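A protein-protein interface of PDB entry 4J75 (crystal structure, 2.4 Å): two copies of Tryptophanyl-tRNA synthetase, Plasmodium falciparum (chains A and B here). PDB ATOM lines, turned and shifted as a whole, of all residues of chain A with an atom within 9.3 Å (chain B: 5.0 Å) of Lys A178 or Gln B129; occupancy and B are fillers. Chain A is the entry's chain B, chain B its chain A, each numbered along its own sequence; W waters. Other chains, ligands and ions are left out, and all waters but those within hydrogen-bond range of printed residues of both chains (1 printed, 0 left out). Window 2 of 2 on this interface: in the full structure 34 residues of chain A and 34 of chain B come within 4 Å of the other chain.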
ATOM      1  N   TYR A 170      -1.883  34.004   1.640  1.00  0.00           N
ATOM      2  CA  TYR A 170      -1.532  32.758   0.937  1.00  0.00           C
ATOM      3  C   TYR A 170      -0.636  31.801   1.738  1.00  0.00           C
ATOM      4  O   TYR A 170      -0.916  30.601   1.782  1.00  0.00           O
ATOM      5  CB  TYR A 170      -0.930  33.058  -0.423  1.00  0.00           C
ATOM      6  CG  TYR A 170      -0.791  31.855  -1.348  1.00  0.00           C
ATOM      7  CD1 TYR A 170      -1.864  31.013  -1.602  1.00  0.00           C
ATOM      8  CD2 TYR A 170       0.403  31.608  -2.010  1.00  0.00           C
ATOM      9  CE1 TYR A 170      -1.737  29.937  -2.464  1.00  0.00           C
ATOM     10  CE2 TYR A 170       0.539  30.541  -2.869  1.00  0.00           C
ATOM     11  CZ  TYR A 170      -0.530  29.702  -3.095  1.00  0.00           C
ATOM     12  OH  TYR A 170      -0.396  28.643  -3.965  1.00  0.00           O
ATOM     13  N   PRO A 171       0.420  32.315   2.392  1.00  0.00           N
ATOM     14  CA  PRO A 171       1.234  31.381   3.196  1.00  0.00           C
ATOM     15  C   PRO A 171       0.418  30.606   4.225  1.00  0.00           C
ATOM     16  O   PRO A 171       0.640  29.429   4.426  1.00  0.00           O
ATOM     17  CB  PRO A 171       2.245  32.307   3.880  1.00  0.00           C
ATOM     18  CG  PRO A 171       2.452  33.383   2.865  1.00  0.00           C
ATOM     19  CD  PRO A 171       1.068  33.633   2.295  1.00  0.00           C
ATOM     20  N   THR A 172      -0.560  31.270   4.817  1.00  0.00           N
ATOM     21  CA  THR A 172      -1.398  30.638   5.806  1.00  0.00           C
ATOM     22  C   THR A 172      -2.370  29.673   5.121  1.00  0.00           C
ATOM     23  O   THR A 172      -2.564  28.541   5.591  1.00  0.00           O
ATOM     24  CB  THR A 172      -2.146  31.697   6.608  1.00  0.00           C
ATOM     25  OG1 THR A 172      -1.195  32.545   7.236  1.00  0.00           O
ATOM     26  CG2 THR A 172      -3.012  31.056   7.660  1.00  0.00           C
ATOM     27  N   VAL A 173      -2.940  30.117   4.001  1.00  0.00           N
ATOM     28  CA  VAL A 173      -3.799  29.277   3.176  1.00  0.00           C
ATOM     29  C   VAL A 173      -3.082  27.976   2.800  1.00  0.00           C
ATOM     30  O   VAL A 173      -3.680  26.904   2.836  1.00  0.00           O
ATOM     31  CB  VAL A 173      -4.240  30.022   1.892  1.00  0.00           C
ATOM     32  CG1 VAL A 173      -4.859  29.075   0.890  1.00  0.00           C
ATOM     33  CG2 VAL A 173      -5.206  31.142   2.236  1.00  0.00           C
ATOM     34  N   LEU A 174      -1.804  28.077   2.449  1.00  0.00           N
ATOM     35  CA  LEU A 174      -1.020  26.899   2.058  1.00  0.00           C
ATOM     36  C   LEU A 174      -0.991  25.870   3.169  1.00  0.00           C
ATOM     37  O   LEU A 174      -1.172  24.681   2.936  1.00  0.00           O
ATOM     38  CB  LEU A 174       0.415  27.292   1.682  1.00  0.00           C
ATOM     39  CG  LEU A 174       0.528  27.967   0.311  1.00  0.00           C
ATOM     40  CD1 LEU A 174       1.953  28.456   0.066  1.00  0.00           C
ATOM     41  CD2 LEU A 174       0.076  27.029  -0.808  1.00  0.00           C
ATOM     42  N   SER A 175      -0.759  26.334   4.386  1.00  0.00           N
ATOM     43  CA  SER A 175      -0.699  25.438   5.514  1.00  0.00           C
ATOM     44  C   SER A 175      -2.064  24.794   5.798  1.00  0.00           C
ATOM     45  O   SER A 175      -2.139  23.613   6.145  1.00  0.00           O
ATOM     46  CB  SER A 175      -0.188  26.168   6.728  1.00  0.00           C
ATOM     47  OG  SER A 175      -0.164  25.260   7.814  1.00  0.00           O
ATOM     48  N   ILE A 176      -3.130  25.576   5.638  1.00  0.00           N
ATOM     49  CA  ILE A 176      -4.496  25.090   5.819  1.00  0.00           C
ATOM     50  C   ILE A 176      -4.833  24.069   4.720  1.00  0.00           C
ATOM     51  O   ILE A 176      -5.333  22.987   5.008  1.00  0.00           O
ATOM     52  CB  ILE A 176      -5.503  26.262   5.802  1.00  0.00           C
ATOM     53  CG1 ILE A 176      -5.277  27.179   7.006  1.00  0.00           C
ATOM     54  CG2 ILE A 176      -6.932  25.752   5.824  1.00  0.00           C
ATOM     55  CD1 ILE A 176      -5.842  28.566   6.807  1.00  0.00           C
ATOM     56  N   HIS A 177      -4.515  24.412   3.470  1.00  0.00           N
ATOM     57  CA  HIS A 177      -4.644  23.483   2.347  1.00  0.00           C
ATOM     58  C   HIS A 177      -3.988  22.152   2.664  1.00  0.00           C
ATOM     59  O   HIS A 177      -4.599  21.088   2.482  1.00  0.00           O
ATOM     60  CB  HIS A 177      -3.972  24.017   1.071  1.00  0.00           C
ATOM     61  CG  HIS A 177      -4.781  25.018   0.294  1.00  0.00           C
ATOM     62  ND1 HIS A 177      -6.121  25.246   0.512  1.00  0.00           N
ATOM     63  CD2 HIS A 177      -4.426  25.840  -0.723  1.00  0.00           C
ATOM     64  CE1 HIS A 177      -6.549  26.183  -0.316  1.00  0.00           C
ATOM     65  NE2 HIS A 177      -5.543  26.550  -1.086  1.00  0.00           N
ATOM     66  N   LYS A 178      -2.736  22.212   3.106  1.00  0.00           N
ATOM     67  CA  LYS A 178      -1.938  21.006   3.305  1.00  0.00           C
ATOM     68  C   LYS A 178      -2.597  20.079   4.328  1.00  0.00           C
ATOM     69  O   LYS A 178      -2.499  18.867   4.232  1.00  0.00           O
ATOM     70  CB  LYS A 178      -0.515  21.366   3.747  1.00  0.00           C
ATOM     71  CG  LYS A 178       0.489  20.238   3.586  1.00  0.00           C
ATOM     72  CD  LYS A 178       1.924  20.713   3.808  1.00  0.00           C
ATOM     73  CE  LYS A 178       2.911  19.563   3.652  1.00  0.00           C
ATOM     74  NZ  LYS A 178       4.324  19.999   3.806  1.00  0.00           N
ATOM     75  N   LYS A 179      -3.299  20.680   5.280  1.00  0.00           N
ATOM     76  CA  LYS A 179      -3.931  19.943   6.353  1.00  0.00           C
ATOM     77  C   LYS A 179      -5.414  19.646   6.089  1.00  0.00           C
ATOM     78  O   LYS A 179      -6.157  19.320   7.013  1.00  0.00           O
ATOM     79  CB  LYS A 179      -3.759  20.734   7.649  1.00  0.00           C
ATOM     80  CG  LYS A 179      -2.300  20.862   8.049  1.00  0.00           C
ATOM     81  CD  LYS A 179      -2.082  21.984   9.048  1.00  0.00           C
ATOM     82  CE  LYS A 179      -0.606  22.101   9.411  1.00  0.00           C
ATOM     83  NZ  LYS A 179       0.243  22.456   8.239  1.00  0.00           N
ATOM     84  N   THR A 180      -5.831  19.745   4.830  1.00  0.00           N
ATOM     85  CA  THR A 180      -7.204  19.443   4.429  1.00  0.00           C
ATOM     86  C   THR A 180      -7.224  18.515   3.224  1.00  0.00           C
ATOM     87  O   THR A 180      -6.932  18.939   2.101  1.00  0.00           O
ATOM     88  CB  THR A 180      -7.967  20.736   4.059  1.00  0.00           C
ATOM     89  OG1 THR A 180      -7.890  21.678   5.133  1.00  0.00           O
ATOM     90  CG2 THR A 180      -9.423  20.428   3.762  1.00  0.00           C
ATOM     91  N   THR A 181      -7.565  17.254   3.445  1.00  0.00           N
ATOM     92  CA  THR A 181      -7.702  16.307   2.339  1.00  0.00           C
ATOM     93  C   THR A 181      -8.900  16.687   1.491  1.00  0.00           C
ATOM     94  O   THR A 181      -9.811  17.365   1.949  1.00  0.00           O
ATOM     95  CB  THR A 181      -7.893  14.856   2.821  1.00  0.00           C
ATOM     96  OG1 THR A 181      -9.163  14.732   3.467  1.00  0.00           O
ATOM     97  CG2 THR A 181      -6.766  14.422   3.781  1.00  0.00           C
ATOM     98  N   LEU A 182      -8.897  16.246   0.245  1.00  0.00           N
ATOM     99  CA  LEU A 182     -10.033  16.447  -0.624  1.00  0.00           C
ATOM    100  C   LEU A 182     -11.272  15.818  -0.003  1.00  0.00           C
ATOM    101  O   LEU A 182     -12.347  16.401  -0.057  1.00  0.00           O
ATOM    102  CB  LEU A 182      -9.758  15.853  -1.999  1.00  0.00           C
ATOM    103  CG  LEU A 182     -10.878  15.991  -3.031  1.00  0.00           C
ATOM    104  CD1 LEU A 182     -11.266  17.447  -3.224  1.00  0.00           C
ATOM    105  CD2 LEU A 182     -10.453  15.373  -4.348  1.00  0.00           C
ATOM    106  N   GLN A 184     -12.029  15.499   3.179  1.00  0.00           N
ATOM    107  CA  GLN A 184     -12.562  16.389   4.204  1.00  0.00           C
ATOM    108  C   GLN A 184     -13.340  17.552   3.600  1.00  0.00           C
ATOM    109  O   GLN A 184     -14.436  17.859   4.059  1.00  0.00           O
ATOM    110  CB  GLN A 184     -11.455  16.991   5.026  1.00  0.00           C
ATOM    111  CG  GLN A 184     -10.856  16.117   6.087  1.00  0.00           C
ATOM    112  CD  GLN A 184      -9.893  16.933   6.923  1.00  0.00           C
ATOM    113  OE1 GLN A 184     -10.331  17.772   7.710  1.00  0.00           O
ATOM    114  NE2 GLN A 184      -8.577  16.722   6.733  1.00  0.00           N
ATOM    115  N   SER A 204     -10.258  27.524   2.705  1.00  0.00           N
ATOM    116  CA  SER A 204      -9.010  27.844   3.372  1.00  0.00           C
ATOM    117  C   SER A 204      -8.830  29.373   3.429  1.00  0.00           C
ATOM    118  O   SER A 204      -8.266  29.905   4.389  1.00  0.00           O
ATOM    119  CB  SER A 204      -7.845  27.182   2.649  1.00  0.00           C
ATOM    120  OG  SER A 204      -7.983  25.763   2.603  1.00  0.00           O
ATOM    121  N   ILE A 243      -7.646  22.442  12.446  1.00  0.00           N
ATOM    122  CA  ILE A 243      -6.448  22.818  11.707  1.00  0.00           C
ATOM    123  C   ILE A 243      -5.538  23.707  12.545  1.00  0.00           C
ATOM    124  O   ILE A 243      -4.320  23.577  12.484  1.00  0.00           O
ATOM    125  CB  ILE A 243      -6.810  23.468  10.356  1.00  0.00           C
ATOM    126  CG1 ILE A 243      -7.590  22.400   9.556  1.00  0.00           C
ATOM    127  CG2 ILE A 243      -5.578  23.987   9.604  1.00  0.00           C
ATOM    128  CD1 ILE A 243      -7.574  22.501   8.051  1.00  0.00           C
ATOM    129  N   LYS A 246      -3.211  21.627  14.552  1.00  0.00           N
ATOM    130  CA  LYS A 246      -2.134  21.103  13.724  1.00  0.00           C
ATOM    131  C   LYS A 246      -1.105  22.169  13.349  1.00  0.00           C
ATOM    132  O   LYS A 246       0.084  21.853  13.250  1.00  0.00           O
ATOM    133  CB  LYS A 246      -2.695  20.470  12.465  1.00  0.00           C
ATOM    134  CG  LYS A 246      -3.524  19.223  12.726  1.00  0.00           C
ATOM    135  CD  LYS A 246      -4.036  18.652  11.407  1.00  0.00           C
ATOM    136  CE  LYS A 246      -5.080  17.557  11.589  1.00  0.00           C
ATOM    137  NZ  LYS A 246      -5.592  17.135  10.248  1.00  0.00           N
ATOM    138  N   MET A 247      -1.555  23.421  13.207  1.00  0.00           N
ATOM    139  CA  MET A 247      -0.658  24.563  12.945  1.00  0.00           C
ATOM    140  C   MET A 247      -0.013  25.125  14.197  1.00  0.00           C
ATOM    141  O   MET A 247       0.797  26.050  14.107  1.00  0.00           O
ATOM    142  CB  MET A 247      -1.404  25.701  12.228  1.00  0.00           C
ATOM    143  CG  MET A 247      -1.901  25.327  10.846  1.00  0.00           C
ATOM    144  SD  MET A 247      -2.618  26.679   9.876  1.00  0.00           S
ATOM    145  CE  MET A 247      -3.994  27.188  10.887  1.00  0.00           C
ATOM    146  N   TYR B 125       6.088  22.637  -1.133  1.00  0.00           N
ATOM    147  CA  TYR B 125       5.596  22.586   0.241  1.00  0.00           C
ATOM    148  C   TYR B 125       4.392  21.673   0.318  1.00  0.00           C
ATOM    149  O   TYR B 125       4.304  20.821   1.202  1.00  0.00           O
ATOM    150  CB  TYR B 125       5.195  23.982   0.737  1.00  0.00           C
ATOM    151  CG  TYR B 125       4.432  23.941   2.040  1.00  0.00           C
ATOM    152  CD1 TYR B 125       5.031  23.476   3.195  1.00  0.00           C
ATOM    153  CD2 TYR B 125       3.113  24.387   2.112  1.00  0.00           C
ATOM    154  CE1 TYR B 125       4.356  23.457   4.392  1.00  0.00           C
ATOM    155  CE2 TYR B 125       2.421  24.372   3.309  1.00  0.00           C
ATOM    156  CZ  TYR B 125       3.045  23.910   4.443  1.00  0.00           C
ATOM    157  OH  TYR B 125       2.354  23.877   5.626  1.00  0.00           O
ATOM    158  N   LEU B 126       3.467  21.863  -0.620  1.00  0.00           N
ATOM    159  CA  LEU B 126       2.221  21.103  -0.641  1.00  0.00           C
ATOM    160  C   LEU B 126       2.385  19.630  -0.997  1.00  0.00           C
ATOM    161  O   LEU B 126       1.604  18.789  -0.519  1.00  0.00           O
ATOM    162  CB  LEU B 126       1.242  21.733  -1.622  1.00  0.00           C
ATOM    163  CG  LEU B 126       0.681  23.085  -1.208  1.00  0.00           C
ATOM    164  CD1 LEU B 126      -0.028  23.687  -2.405  1.00  0.00           C
ATOM    165  CD2 LEU B 126      -0.235  22.962   0.000  1.00  0.00           C
ATOM    166  N   PHE B 127       3.374  19.309  -1.830  1.00  0.00           N
ATOM    167  CA  PHE B 127       3.556  17.923  -2.276  1.00  0.00           C
ATOM    168  C   PHE B 127       4.444  17.078  -1.361  1.00  0.00           C
ATOM    169  O   PHE B 127       4.406  15.863  -1.458  1.00  0.00           O
ATOM    170  CB  PHE B 127       4.069  17.867  -3.723  1.00  0.00           C
ATOM    171  CG  PHE B 127       2.986  18.115  -4.762  1.00  0.00           C
ATOM    172  CD1 PHE B 127       2.433  19.376  -4.926  1.00  0.00           C
ATOM    173  CD2 PHE B 127       2.516  17.070  -5.572  1.00  0.00           C
ATOM    174  CE1 PHE B 127       1.452  19.616  -5.870  1.00  0.00           C
ATOM    175  CE2 PHE B 127       1.523  17.300  -6.528  1.00  0.00           C
ATOM    176  CZ  PHE B 127       0.984  18.580  -6.672  1.00  0.00           C
ATOM    177  N   ASN B 128       5.231  17.706  -0.485  1.00  0.00           N
ATOM    178  CA  ASN B 128       6.157  16.964   0.381  1.00  0.00           C
ATOM    179  C   ASN B 128       5.715  17.088   1.830  1.00  0.00           C
ATOM    180  O   ASN B 128       5.878  18.146   2.449  1.00  0.00           O
ATOM    181  CB  ASN B 128       7.583  17.470   0.211  1.00  0.00           C
ATOM    182  CG  ASN B 128       8.155  17.165  -1.166  1.00  0.00           C
ATOM    183  OD1 ASN B 128       8.605  16.065  -1.426  1.00  0.00           O
ATOM    184  ND2 ASN B 128       8.161  18.145  -2.033  1.00  0.00           N
ATOM    185  N   GLN B 129       5.156  16.006   2.369  1.00  0.00           N
ATOM    186  CA  GLN B 129       4.429  16.069   3.635  1.00  0.00           C
ATOM    187  C   GLN B 129       5.267  16.562   4.823  1.00  0.00           C
ATOM    188  O   GLN B 129       4.754  17.265   5.695  1.00  0.00           O
ATOM    189  CB  GLN B 129       3.800  14.703   3.964  1.00  0.00           C
ATOM    190  CG  GLN B 129       2.881  14.700   5.191  1.00  0.00           C
ATOM    191  CD  GLN B 129       1.721  15.694   5.080  1.00  0.00           C
ATOM    192  OE1 GLN B 129       1.246  15.989   3.974  1.00  0.00           O
ATOM    193  NE2 GLN B 129       1.267  16.225   6.224  1.00  0.00           N
ATOM    194  N   ASN B 130       6.546  16.202   4.843  1.00  0.00           N
ATOM    195  CA  ASN B 130       7.428  16.528   5.966  1.00  0.00           C
ATOM    196  C   ASN B 130       8.247  17.809   5.792  1.00  0.00           C
ATOM    197  O   ASN B 130       9.049  18.142   6.658  1.00  0.00           O
ATOM    198  CB  ASN B 130       8.362  15.350   6.237  1.00  0.00           C
ATOM    199  CG  ASN B 130       7.603  14.083   6.587  1.00  0.00           C
ATOM    200  OD1 ASN B 130       6.548  14.124   7.236  1.00  0.00           O
ATOM    201  ND2 ASN B 130       8.137  12.951   6.168  1.00  0.00           N
ATOM    202  N   TYR B 131       8.032  18.530   4.694  1.00  0.00           N
ATOM    203  CA  TYR B 131       8.774  19.756   4.420  1.00  0.00           C
ATOM    204  C   TYR B 131       7.988  20.968   4.904  1.00  0.00           C
ATOM    205  O   TYR B 131       6.810  21.140   4.553  1.00  0.00           O
ATOM    206  CB  TYR B 131       9.032  19.888   2.931  1.00  0.00           C
ATOM    207  CG  TYR B 131      10.048  18.944   2.325  1.00  0.00           C
ATOM    208  CD1 TYR B 131      10.612  17.896   3.043  1.00  0.00           C
ATOM    209  CD2 TYR B 131      10.423  19.094   0.989  1.00  0.00           C
ATOM    210  CE1 TYR B 131      11.534  17.041   2.456  1.00  0.00           C
ATOM    211  CE2 TYR B 131      11.341  18.249   0.393  1.00  0.00           C
ATOM    212  CZ  TYR B 131      11.890  17.223   1.122  1.00  0.00           C
ATOM    213  OH  TYR B 131      12.798  16.381   0.513  1.00  0.00           O
ATOM    214  N   ASN B 196      -4.178  16.483  -0.442  1.00  0.00           N
ATOM    215  CA  ASN B 196      -4.641  17.727   0.117  1.00  0.00           C
ATOM    216  C   ASN B 196      -5.127  18.677  -0.982  1.00  0.00           C
ATOM    217  O   ASN B 196      -4.713  18.586  -2.138  1.00  0.00           O
ATOM    218  CB  ASN B 196      -3.575  18.362   1.024  1.00  0.00           C
ATOM    219  CG  ASN B 196      -2.382  18.882   0.260  1.00  0.00           C
ATOM    220  OD1 ASN B 196      -2.473  19.862  -0.485  1.00  0.00           O
ATOM    221  ND2 ASN B 196      -1.245  18.245   0.465  1.00  0.00           N
HETATM  222  O   HOH W   1       3.090  22.728   7.889  1.00  0.00           O
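The backbone carbonyl oxygen (O) of Tyr B131 is in hydrogen-bond range of the side-chain amino group (NZ) of Lys A178.
O of Tyr B125 lies within hydrogen-bond range of NZ of Lys A178, 2.7 Å away.
NZ of Lys A178 is in hydrogen-bond range of O of Asn B128 (2.8 Å).
O of Gln B129 is in hydrogen-bond range of NZ of Lys A178, 3.4 Å away.
O of Ile A176 is in hydrogen-bond range of OG1 of Thr A180, at 2.9 Å.
The side-chain hydroxyl (OG) of Ser A175 is in hydrogen-bond range of the side-chain amino group (NZ) of Lys A179.
OG of Ser A175 lies close to SD of Met A247 (3.5 Å).
The side-chain amide nitrogen of Asn B196 sits at hydrogen-bond distance from the backbone carbonyl oxygen of Leu B126.
A ring nitrogen (ND1) of His A177 sits at hydrogen-bond distance from the side-chain hydroxyl (OG) of Ser A204 (2.8 Å).
Among the printed residues, merely in contact across the chains: Leu A174 with Tyr B125, Leu A174 with Leu B126, Ser A175 with Tyr B125, His A177 with Asn B196, Lys A178 with Asn B196, Lys A179 with Tyr B125 and Thr A180 with Asn B196.
Tyr A170 touches none of the printed residues of chain B.
Pro A171 touches none of the printed residues of chain B.
Printed residues of chain B within 4 Å of Leu A174: Tyr B125 (3.6 Å) and Leu B126 (3.5 Å).
Printed residues of chain B within 4 Å of His A177: Asn B196.
Of chain B, only Tyr B125 (2.7 Å), Asn B128 (2.8 Å), Gln B129 (3.4 Å), Tyr B131 (2.8 Å) and Asn B196 (3.4 Å) come within 4 Å of Lys A178.
Of the printed residues of chain B, Lys A179 touches Tyr B125 (3.6 Å).
Printed residues of chain A within 4 Å of Asn B128: Lys A178 (2.8 Å).
Of chain A, only Lys A178 comes within 4 Å of Gln B129.
No residue of chain A comes within 4 Å of Asn B130.
The nearest residue of chain A that does not touch Gln B129 is Lys A179 (6.1 Å).
Printed residues of chain A that touch a printed residue of chain B: Leu A174, Ser A175, His A177, Lys A178, Lys A179 and Thr A180.
Hydrophobic or aromatic side chains of chain A within 4 Å of the printed part of chain B: Leu A174.
Of the 8 printed residues of chain B, 6 touch a printed residue of chain A.
Among the printed residues, no Asp or Glu carboxylate lies within 4 Å of a Lys or Arg side-chain nitrogen of the other chain.
No position is printed for both chains.
Of the 11 pairs that touch across the chains among the printed residues, none has its exchanged pair printed and touching as well.
Water W1 bridges the side-chain hydroxyl (OH) of Tyr B125 and the side-chain amino group (NZ) of Lys A179.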
